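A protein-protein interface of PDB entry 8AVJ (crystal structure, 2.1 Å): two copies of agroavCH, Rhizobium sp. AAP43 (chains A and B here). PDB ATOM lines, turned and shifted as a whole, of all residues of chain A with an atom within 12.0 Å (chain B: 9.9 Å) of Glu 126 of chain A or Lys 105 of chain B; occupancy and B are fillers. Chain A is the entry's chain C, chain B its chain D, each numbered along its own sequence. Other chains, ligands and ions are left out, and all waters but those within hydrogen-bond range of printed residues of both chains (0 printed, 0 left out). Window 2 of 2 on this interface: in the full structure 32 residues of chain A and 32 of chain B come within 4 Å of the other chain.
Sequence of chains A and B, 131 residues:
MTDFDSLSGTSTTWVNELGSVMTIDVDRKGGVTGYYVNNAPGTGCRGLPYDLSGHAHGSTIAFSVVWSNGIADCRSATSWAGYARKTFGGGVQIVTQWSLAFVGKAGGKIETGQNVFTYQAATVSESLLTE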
ATOM      1  N   ALA A 122     -27.028  14.899 -14.766  1.00  0.00           N
ATOM      2  CA  ALA A 122     -26.554  16.060 -14.002  1.00  0.00           C
ATOM      3  C   ALA A 122     -27.448  16.286 -12.779  1.00  0.00           C
ATOM      4  O   ALA A 122     -28.640  16.042 -12.881  1.00  0.00           O
ATOM      5  CB  ALA A 122     -26.531  17.279 -14.913  1.00  0.00           C
ATOM      6  N   THR A 123     -26.874  16.784 -11.678  1.00  0.00           N
ATOM      7  CA  THR A 123     -27.597  17.189 -10.452  1.00  0.00           C
ATOM      8  C   THR A 123     -27.358  18.666 -10.137  1.00  0.00           C
ATOM      9  O   THR A 123     -26.297  19.254 -10.571  1.00  0.00           O
ATOM     10  CB  THR A 123     -27.172  16.380  -9.222  1.00  0.00           C
ATOM     11  OG1 THR A 123     -25.801  16.662  -8.989  1.00  0.00           O
ATOM     12  CG2 THR A 123     -27.342  14.887  -9.409  1.00  0.00           C
ATOM     13  N   VAL A 124     -28.312  19.224  -9.396  1.00  0.00           N
ATOM     14  CA  VAL A 124     -28.305  20.620  -8.885  1.00  0.00           C
ATOM     15  C   VAL A 124     -28.570  20.522  -7.393  1.00  0.00           C
ATOM     16  O   VAL A 124     -29.573  19.922  -7.060  1.00  0.00           O
ATOM     17  CB  VAL A 124     -29.407  21.466  -9.544  1.00  0.00           C
ATOM     18  CG1 VAL A 124     -29.300  22.929  -9.124  1.00  0.00           C
ATOM     19  CG2 VAL A 124     -29.459  21.310 -11.058  1.00  0.00           C
ATOM     20  N   SER A 125     -27.721  21.096  -6.550  1.00  0.00           N
ATOM     21  CA  SER A 125     -27.972  21.275  -5.100  1.00  0.00           C
ATOM     22  C   SER A 125     -28.372  22.728  -4.839  1.00  0.00           C
ATOM     23  O   SER A 125     -28.282  23.592  -5.768  1.00  0.00           O
ATOM     24  CB  SER A 125     -26.781  20.911  -4.288  1.00  0.00           C
ATOM     25  OG  SER A 125     -26.423  19.574  -4.541  1.00  0.00           O
ATOM     26  N   GLU A 126     -28.817  22.987  -3.613  1.00  0.00           N
ATOM     27  CA  GLU A 126     -29.188  24.346  -3.175  1.00  0.00           C
ATOM     28  C   GLU A 126     -27.907  25.184  -3.093  1.00  0.00           C
ATOM     29  O   GLU A 126     -27.905  26.272  -3.644  1.00  0.00           O
ATOM     30  CB  GLU A 126     -29.916  24.313  -1.835  1.00  0.00           C
ATOM     31  CG  GLU A 126     -30.245  25.707  -1.345  1.00  0.00           C
ATOM     32  CD  GLU A 126     -31.098  25.680  -0.103  1.00  0.00           C
ATOM     33  OE1 GLU A 126     -30.520  25.830   0.991  1.00  0.00           O
ATOM     34  OE2 GLU A 126     -32.317  25.458  -0.248  1.00  0.00           O
ATOM     35  N   SER A 127     -26.882  24.655  -2.430  1.00  0.00           N
ATOM     36  CA  SER A 127     -25.612  25.324  -2.067  1.00  0.00           C
ATOM     37  C   SER A 127     -24.510  24.262  -1.971  1.00  0.00           C
ATOM     38  O   SER A 127     -24.821  23.059  -1.970  1.00  0.00           O
ATOM     39  CB  SER A 127     -25.778  26.141  -0.781  1.00  0.00           C
ATOM     40  OG  SER A 127     -25.226  25.498   0.353  1.00  0.00           O
ATOM     41  N   LEU A 128     -23.255  24.692  -1.884  1.00  0.00           N
ATOM     42  CA  LEU A 128     -22.099  23.793  -1.668  1.00  0.00           C
ATOM     43  C   LEU A 128     -22.208  23.065  -0.308  1.00  0.00           C
ATOM     44  O   LEU A 128     -21.448  22.094  -0.121  1.00  0.00           O
ATOM     45  CB  LEU A 128     -20.831  24.645  -1.718  1.00  0.00           C
ATOM     46  CG  LEU A 128     -19.518  23.878  -1.685  1.00  0.00           C
ATOM     47  CD1 LEU A 128     -19.384  23.006  -2.920  1.00  0.00           C
ATOM     48  CD2 LEU A 128     -18.328  24.821  -1.569  1.00  0.00           C
ATOM     49  N   LEU A 129     -23.037  23.558   0.626  1.00  0.00           N
ATOM     50  CA  LEU A 129     -23.136  23.076   2.039  1.00  0.00           C
ATOM     51  C   LEU A 129     -24.437  22.282   2.255  1.00  0.00           C
ATOM     52  O   LEU A 129     -24.420  21.353   3.069  1.00  0.00           O
ATOM     53  CB  LEU A 129     -23.066  24.283   2.991  1.00  0.00           C
ATOM     54  CG  LEU A 129     -21.831  25.173   2.854  1.00  0.00           C
ATOM     55  CD1 LEU A 129     -21.886  26.339   3.823  1.00  0.00           C
ATOM     56  CD2 LEU A 129     -20.544  24.390   3.042  1.00  0.00           C
ATOM     57  N   THR A 130     -25.526  22.655   1.575  1.00  0.00           N
ATOM     58  CA  THR A 130     -26.892  22.090   1.756  1.00  0.00           C
ATOM     59  C   THR A 130     -27.373  21.577   0.387  1.00  0.00           C
ATOM     60  O   THR A 130     -27.296  22.347  -0.590  1.00  0.00           O
ATOM     61  CB  THR A 130     -27.843  23.097   2.453  1.00  0.00           C
ATOM     62  OG1 THR A 130     -28.554  23.919   1.526  1.00  0.00           O
ATOM     63  CG2 THR A 130     -27.169  24.045   3.428  1.00  0.00           C
ATOM     64  N   GLU A 131     -27.814  20.316   0.306  1.00  0.00           N
ATOM     65  CA  GLU A 131     -28.499  19.720  -0.882  1.00  0.00           C
ATOM     66  C   GLU A 131     -29.960  20.197  -0.924  1.00  0.00           C
ATOM     67  O   GLU A 131     -30.418  20.720  -1.947  1.00  0.00           O
ATOM     68  CB  GLU A 131     -28.395  18.189  -0.847  1.00  0.00           C
ATOM     69  CG  GLU A 131     -26.964  17.683  -1.013  1.00  0.00           C
ATOM     70  CD  GLU A 131     -26.625  16.315  -0.429  1.00  0.00           C
ATOM     71  OE1 GLU A 131     -27.523  15.434  -0.388  1.00  0.00           O
ATOM     72  OE2 GLU A 131     -25.446  16.127  -0.021  1.00  0.00           O
ATOM     73  N   GLY B  44     -21.183  19.512  -1.039  1.00  0.00           N
ATOM     74  CA  GLY B  44     -21.475  18.908  -2.352  1.00  0.00           C
ATOM     75  C   GLY B  44     -20.334  19.119  -3.347  1.00  0.00           C
ATOM     76  O   GLY B  44     -19.199  19.531  -2.940  1.00  0.00           O
ATOM     77  N   CYS B  45     -20.580  18.786  -4.610  1.00  0.00           N
ATOM     78  CA  CYS B  45     -19.590  18.924  -5.726  1.00  0.00           C
ATOM     79  C   CYS B  45     -18.233  18.389  -5.308  1.00  0.00           C
ATOM     80  O   CYS B  45     -17.184  19.082  -5.560  1.00  0.00           O
ATOM     81  CB  CYS B  45     -19.483  20.393  -6.116  1.00  0.00           C
ATOM     82  SG  CYS B  45     -21.098  21.016  -6.617  1.00  0.00           S
ATOM     83  N   TRP B  67     -18.954  26.505  -8.813  1.00  0.00           N
ATOM     84  CA  TRP B  67     -19.279  25.091  -8.482  1.00  0.00           C
ATOM     85  C   TRP B  67     -20.347  24.555  -9.431  1.00  0.00           C
ATOM     86  O   TRP B  67     -21.360  24.063  -8.953  1.00  0.00           O
ATOM     87  CB  TRP B  67     -19.675  24.987  -7.009  1.00  0.00           C
ATOM     88  CG  TRP B  67     -18.499  25.328  -6.153  1.00  0.00           C
ATOM     89  CD1 TRP B  67     -18.356  26.466  -5.421  1.00  0.00           C
ATOM     90  CD2 TRP B  67     -17.263  24.594  -6.003  1.00  0.00           C
ATOM     91  NE1 TRP B  67     -17.145  26.456  -4.787  1.00  0.00           N
ATOM     92  CE2 TRP B  67     -16.444  25.340  -5.142  1.00  0.00           C
ATOM     93  CE3 TRP B  67     -16.755  23.393  -6.504  1.00  0.00           C
ATOM     94  CZ2 TRP B  67     -15.176  24.931  -4.759  1.00  0.00           C
ATOM     95  CZ3 TRP B  67     -15.498  22.979  -6.125  1.00  0.00           C
ATOM     96  CH2 TRP B  67     -14.718  23.745  -5.272  1.00  0.00           C
ATOM     97  N   ALA B  72     -22.424  18.174 -11.420  1.00  0.00           N
ATOM     98  CA  ALA B  72     -23.045  18.644 -10.168  1.00  0.00           C
ATOM     99  C   ALA B  72     -22.915  20.175 -10.082  1.00  0.00           C
ATOM    100  O   ALA B  72     -21.796  20.696 -10.174  1.00  0.00           O
ATOM    101  CB  ALA B  72     -22.387  17.974  -8.993  1.00  0.00           C
ATOM    102  N   ASP B  73     -24.038  20.852  -9.905  1.00  0.00           N
ATOM    103  CA  ASP B  73     -24.123  22.321  -9.736  1.00  0.00           C
ATOM    104  C   ASP B  73     -24.472  22.597  -8.274  1.00  0.00           C
ATOM    105  O   ASP B  73     -25.615  22.359  -7.904  1.00  0.00           O
ATOM    106  CB  ASP B  73     -25.131  22.909 -10.717  1.00  0.00           C
ATOM    107  CG  ASP B  73     -25.290  24.434 -10.636  1.00  0.00           C
ATOM    108  OD1 ASP B  73     -24.692  25.056  -9.742  1.00  0.00           O
ATOM    109  OD2 ASP B  73     -26.030  24.963 -11.450  1.00  0.00           O
ATOM    110  N   CYS B  74     -23.535  23.110  -7.476  1.00  0.00           N
ATOM    111  CA  CYS B  74     -23.844  23.572  -6.094  1.00  0.00           C
ATOM    112  C   CYS B  74     -24.259  25.055  -6.077  1.00  0.00           C
ATOM    113  O   CYS B  74     -24.582  25.534  -4.989  1.00  0.00           O
ATOM    114  CB  CYS B  74     -22.714  23.234  -5.127  1.00  0.00           C
ATOM    115  SG  CYS B  74     -22.456  21.432  -4.928  1.00  0.00           S
ATOM    116  N   ARG B  75     -24.392  25.725  -7.229  1.00  0.00           N
ATOM    117  CA  ARG B  75     -24.898  27.136  -7.305  1.00  0.00           C
ATOM    118  C   ARG B  75     -24.131  28.027  -6.327  1.00  0.00           C
ATOM    119  O   ARG B  75     -24.730  28.782  -5.606  1.00  0.00           O
ATOM    120  CB  ARG B  75     -26.399  27.185  -7.040  1.00  0.00           C
ATOM    121  CG  ARG B  75     -27.198  26.387  -8.066  1.00  0.00           C
ATOM    122  CD  ARG B  75     -28.695  26.455  -7.896  1.00  0.00           C
ATOM    123  NE  ARG B  75     -28.969  26.623  -6.470  1.00  0.00           N
ATOM    124  CZ  ARG B  75     -30.086  27.133  -5.950  1.00  0.00           C
ATOM    125  NH1 ARG B  75     -30.202  27.278  -4.637  1.00  0.00           N
ATOM    126  NH2 ARG B  75     -31.076  27.502  -6.742  1.00  0.00           N
ATOM    127  N   SER B  76     -22.816  27.895  -6.283  1.00  0.00           N
ATOM    128  CA  SER B  76     -21.942  28.605  -5.327  1.00  0.00           C
ATOM    129  C   SER B  76     -20.660  29.025  -6.049  1.00  0.00           C
ATOM    130  O   SER B  76     -20.386  28.497  -7.139  1.00  0.00           O
ATOM    131  CB  SER B  76     -21.665  27.731  -4.129  1.00  0.00           C
ATOM    132  OG  SER B  76     -22.893  27.159  -3.678  1.00  0.00           O
ATOM    133  N   ALA B  77     -19.864  29.883  -5.425  1.00  0.00           N
ATOM    134  CA  ALA B  77     -18.601  30.348  -6.012  1.00  0.00           C
ATOM    135  C   ALA B  77     -17.635  30.541  -4.874  1.00  0.00           C
ATOM    136  O   ALA B  77     -18.048  31.075  -3.836  1.00  0.00           O
ATOM    137  CB  ALA B  77     -18.850  31.589  -6.844  1.00  0.00           C
ATOM    138  N   LEU B 100     -16.721  32.126   0.076  1.00  0.00           N
ATOM    139  CA  LEU B 100     -17.714  31.247  -0.572  1.00  0.00           C
ATOM    140  C   LEU B 100     -19.041  31.979  -0.562  1.00  0.00           C
ATOM    141  O   LEU B 100     -19.488  32.383   0.527  1.00  0.00           O
ATOM    142  CB  LEU B 100     -17.787  29.914   0.190  1.00  0.00           C
ATOM    143  CG  LEU B 100     -19.023  29.058  -0.102  1.00  0.00           C
ATOM    144  CD1 LEU B 100     -18.992  28.500  -1.523  1.00  0.00           C
ATOM    145  CD2 LEU B 100     -19.126  27.926   0.901  1.00  0.00           C
ATOM    146  N   ALA B 101     -19.665  32.106  -1.722  1.00  0.00           N
ATOM    147  CA  ALA B 101     -20.980  32.750  -1.845  1.00  0.00           C
ATOM    148  C   ALA B 101     -21.971  31.706  -2.329  1.00  0.00           C
ATOM    149  O   ALA B 101     -21.576  30.887  -3.181  1.00  0.00           O
ATOM    150  CB  ALA B 101     -20.902  33.906  -2.813  1.00  0.00           C
ATOM    151  N   PHE B 102     -23.195  31.759  -1.803  1.00  0.00           N
ATOM    152  CA  PHE B 102     -24.338  30.888  -2.178  1.00  0.00           C
ATOM    153  C   PHE B 102     -25.634  31.574  -1.751  1.00  0.00           C
ATOM    154  O   PHE B 102     -25.572  32.605  -1.103  1.00  0.00           O
ATOM    155  CB  PHE B 102     -24.170  29.496  -1.558  1.00  0.00           C
ATOM    156  CG  PHE B 102     -23.995  29.465  -0.058  1.00  0.00           C
ATOM    157  CD1 PHE B 102     -22.743  29.619   0.511  1.00  0.00           C
ATOM    158  CD2 PHE B 102     -25.081  29.252   0.783  1.00  0.00           C
ATOM    159  CE1 PHE B 102     -22.574  29.593   1.889  1.00  0.00           C
ATOM    160  CE2 PHE B 102     -24.912  29.212   2.160  1.00  0.00           C
ATOM    161  CZ  PHE B 102     -23.658  29.382   2.712  1.00  0.00           C
ATOM    162  N   VAL B 103     -26.764  31.034  -2.180  1.00  0.00           N
ATOM    163  CA  VAL B 103     -28.131  31.469  -1.769  1.00  0.00           C
ATOM    164  C   VAL B 103     -28.797  30.305  -0.992  1.00  0.00           C
ATOM    165  O   VAL B 103     -29.199  29.314  -1.620  1.00  0.00           O
ATOM    166  CB  VAL B 103     -28.934  31.944  -3.007  1.00  0.00           C
ATOM    167  CG1 VAL B 103     -30.254  32.615  -2.645  1.00  0.00           C
ATOM    168  CG2 VAL B 103     -28.119  32.887  -3.881  1.00  0.00           C
ATOM    169  N   GLY B 104     -28.904  30.405   0.342  1.00  0.00           N
ATOM    170  CA  GLY B 104     -29.785  29.547   1.167  1.00  0.00           C
ATOM    171  C   GLY B 104     -31.252  29.850   0.894  1.00  0.00           C
ATOM    172  O   GLY B 104     -31.533  30.694   0.028  1.00  0.00           O
ATOM    173  N   LYS B 105     -32.181  29.217   1.613  1.00  0.00           N
ATOM    174  CA  LYS B 105     -33.619  29.622   1.588  1.00  0.00           C
ATOM    175  C   LYS B 105     -33.750  30.971   2.309  1.00  0.00           C
ATOM    176  O   LYS B 105     -34.745  31.687   2.053  1.00  0.00           O
ATOM    177  CB  LYS B 105     -34.521  28.543   2.199  1.00  0.00           C
ATOM    178  CG  LYS B 105     -34.770  27.328   1.309  1.00  0.00           C
ATOM    179  CD  LYS B 105     -36.147  26.685   1.481  1.00  0.00           C
ATOM    180  CE  LYS B 105     -36.261  25.313   0.843  1.00  0.00           C
ATOM    181  NZ  LYS B 105     -35.493  24.296   1.605  1.00  0.00           N
ATOM    182  N   ALA B 106     -32.748  31.320   3.126  1.00  0.00           N
ATOM    183  CA  ALA B 106     -32.660  32.570   3.916  1.00  0.00           C
ATOM    184  C   ALA B 106     -32.191  33.757   3.054  1.00  0.00           C
ATOM    185  O   ALA B 106     -32.216  34.882   3.572  1.00  0.00           O
ATOM    186  CB  ALA B 106     -31.728  32.336   5.085  1.00  0.00           C
ATOM    187  N   GLY B 107     -31.784  33.524   1.799  1.00  0.00           N
ATOM    188  CA  GLY B 107     -31.156  34.525   0.907  1.00  0.00           C
ATOM    189  C   GLY B 107     -29.656  34.293   0.791  1.00  0.00           C
ATOM    190  O   GLY B 107     -29.188  33.200   1.157  1.00  0.00           O
ATOM    191  N   GLY B 108     -28.897  35.280   0.313  1.00  0.00           N
ATOM    192  CA  GLY B 108     -27.463  35.092   0.025  1.00  0.00           C
ATOM    193  C   GLY B 108     -26.644  35.064   1.290  1.00  0.00           C
ATOM    194  O   GLY B 108     -27.030  35.719   2.257  1.00  0.00           O
ATOM    195  N   LYS B 109     -25.531  34.349   1.289  1.00  0.00           N
ATOM    196  CA  LYS B 109     -24.582  34.317   2.431  1.00  0.00           C
ATOM    197  C   LYS B 109     -23.206  34.133   1.853  1.00  0.00           C
ATOM    198  O   LYS B 109     -23.112  33.555   0.741  1.00  0.00           O
ATOM    199  CB  LYS B 109     -24.694  33.105   3.371  1.00  0.00           C
ATOM    200  CG  LYS B 109     -26.103  32.635   3.678  1.00  0.00           C
ATOM    201  CD  LYS B 109     -26.799  33.435   4.753  1.00  0.00           C
ATOM    202  CE  LYS B 109     -28.274  33.105   4.848  1.00  0.00           C
ATOM    203  NZ  LYS B 109     -29.010  34.200   5.517  1.00  0.00           N
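The side-chain amino group of Lys 105 of chain B is in salt-bridge range of the side-chain carboxylate of Glu 126 of chain A (3.9 Å).
The backbone carbonyl oxygen of Leu 128 of chain A sits at hydrogen-bond distance from the backbone NH of Gly 44 of chain B (2.8 Å).
The backbone NH (N) of Ser 125 of chain A is in hydrogen-bond range of the backbone carbonyl oxygen (O) of Asp 73 of chain B (2.8 Å).
NH1 of Arg 75 of chain B is in hydrogen-bond range of O of Glu 126 of chain A.
O of Thr 123 of chain A sits at hydrogen-bond distance from N of Asp 73 of chain B (2.8 Å).
The backbone NH of Leu 128 of chain A lies within hydrogen-bond range of the side-chain hydroxyl of Ser 76 of chain B.
The backbone carbonyl oxygen (O) of Ser 125 of chain A lies within hydrogen-bond range of the guanidinium group (NE) of Arg 75 of chain B (3.2 Å).
The backbone carbonyl oxygen of Cys 74 of chain B sits at hydrogen-bond distance from the backbone NH of Leu 128 of chain A, at 3.5 Å.
The backbone carbonyl oxygen of Glu 131 of chain A is in hydrogen-bond range of the backbone NH of Glu 126 of chain A (3.2 Å).
N of Cys 74 of chain B lies within hydrogen-bond range of O of Trp 67 of chain B.
The backbone carbonyl oxygen (O) of Cys 74 of chain B is in hydrogen-bond range of the side-chain hydroxyl (OG) of Ser 76 of chain B (2.7 Å).
The backbone carbonyl oxygen (O) of Phe 102 of chain B lies within hydrogen-bond range of the backbone NH (N) of Lys 109 of chain B.
The side-chain sulfur (SG) of Cys 45 of chain B is disulfide-bonded to the side-chain sulfur (SG) of Cys 74 of chain B (2.2 Å).
The side-chain hydroxyl (OG) of Ser 127 of chain A sits at hydrogen-bond distance from the backbone NH (N) of Thr 130 of chain A.
Among the printed residues, merely in contact across the chains: Ser 127 of chain A with Cys 74 of chain B (3.1 Å), Thr 123 of chain A with Ala 72 of chain B (3.3 Å), Val 124 of chain A with Asp 73 of chain B (3.4 Å), Ser 127 of chain A with Phe 102 of chain B (3.6 Å), Ser 127 of chain A with Ser 76 of chain B (3.7 Å), Glu 126 of chain A with Cys 74 of chain B (3.7 Å), Leu 129 of chain A with Phe 102 of chain B (3.7 Å), Leu 128 of chain A with Leu 100 of chain B (3.7 Å), Glu 126 of chain A with Val 103 of chain B (3.8 Å), Val 124 of chain A with Arg 75 of chain B (3.8 Å), Glu 126 of chain A with Gly 104 of chain B (3.8 Å) and Leu 128 of chain A with Trp 67 of chain B (3.8 Å).
Of the printed residues of chain B, Val 124 of chain A touches Asp 73 (3.4 Å) and Arg 75 (3.8 Å).
Glu 126 of chain A touches just these residues of chain B: Cys 74, Arg 75, Val 103, Gly 104 and Lys 105.
Ser 127 of chain A touches three residues of chain B.
Cys 45 of chain B touches none of the printed residues of chain A.
Of the printed residues of chain A, Ala 72 of chain B touches Thr 123 (3.3 Å).
Arg 75 of chain B touches just these residues of chain A: Val 124 (3.8 Å), Ser 125 (3.2 Å) and Glu 126 (2.7 Å).
Of the printed residues of chain A, Ser 76 of chain B touches Ser 127 (3.7 Å) and Leu 128 (3.1 Å).
Ala 77 of chain B touches none of the printed residues of chain A.
Printed residues of chain A within 4 Å of Lys 105 of chain B: Glu 126.
No residue of chain A comes within 4 Å of Ala 106 of chain B.
No residue of chain A comes within 4 Å of Gly 107 of chain B.
The nearest residue of chain A that does not touch Lys 105 of chain B is Thr 130 of chain A (6.4 Å).
Of the 10 printed residues of chain A, 7 touch a printed residue of chain B.
Hydrophobic or aromatic side chains of chain A that line the printed part of chain B: Val 124, Leu 128 and Leu 129.
Of the 19 printed residues of chain B, 12 touch a printed residue of chain A.
Hydrophobic or aromatic side chains of chain B within 4 Å of the printed part of chain A: Trp 67, Ala 72, Leu 100 and Phe 102.
Among the printed residues, 20 pairs touch across the chains.
No position is printed for both chains.
Of the 20 pairs that touch across the chains among the printed residues, none has its exchanged pair printed and touching as well.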
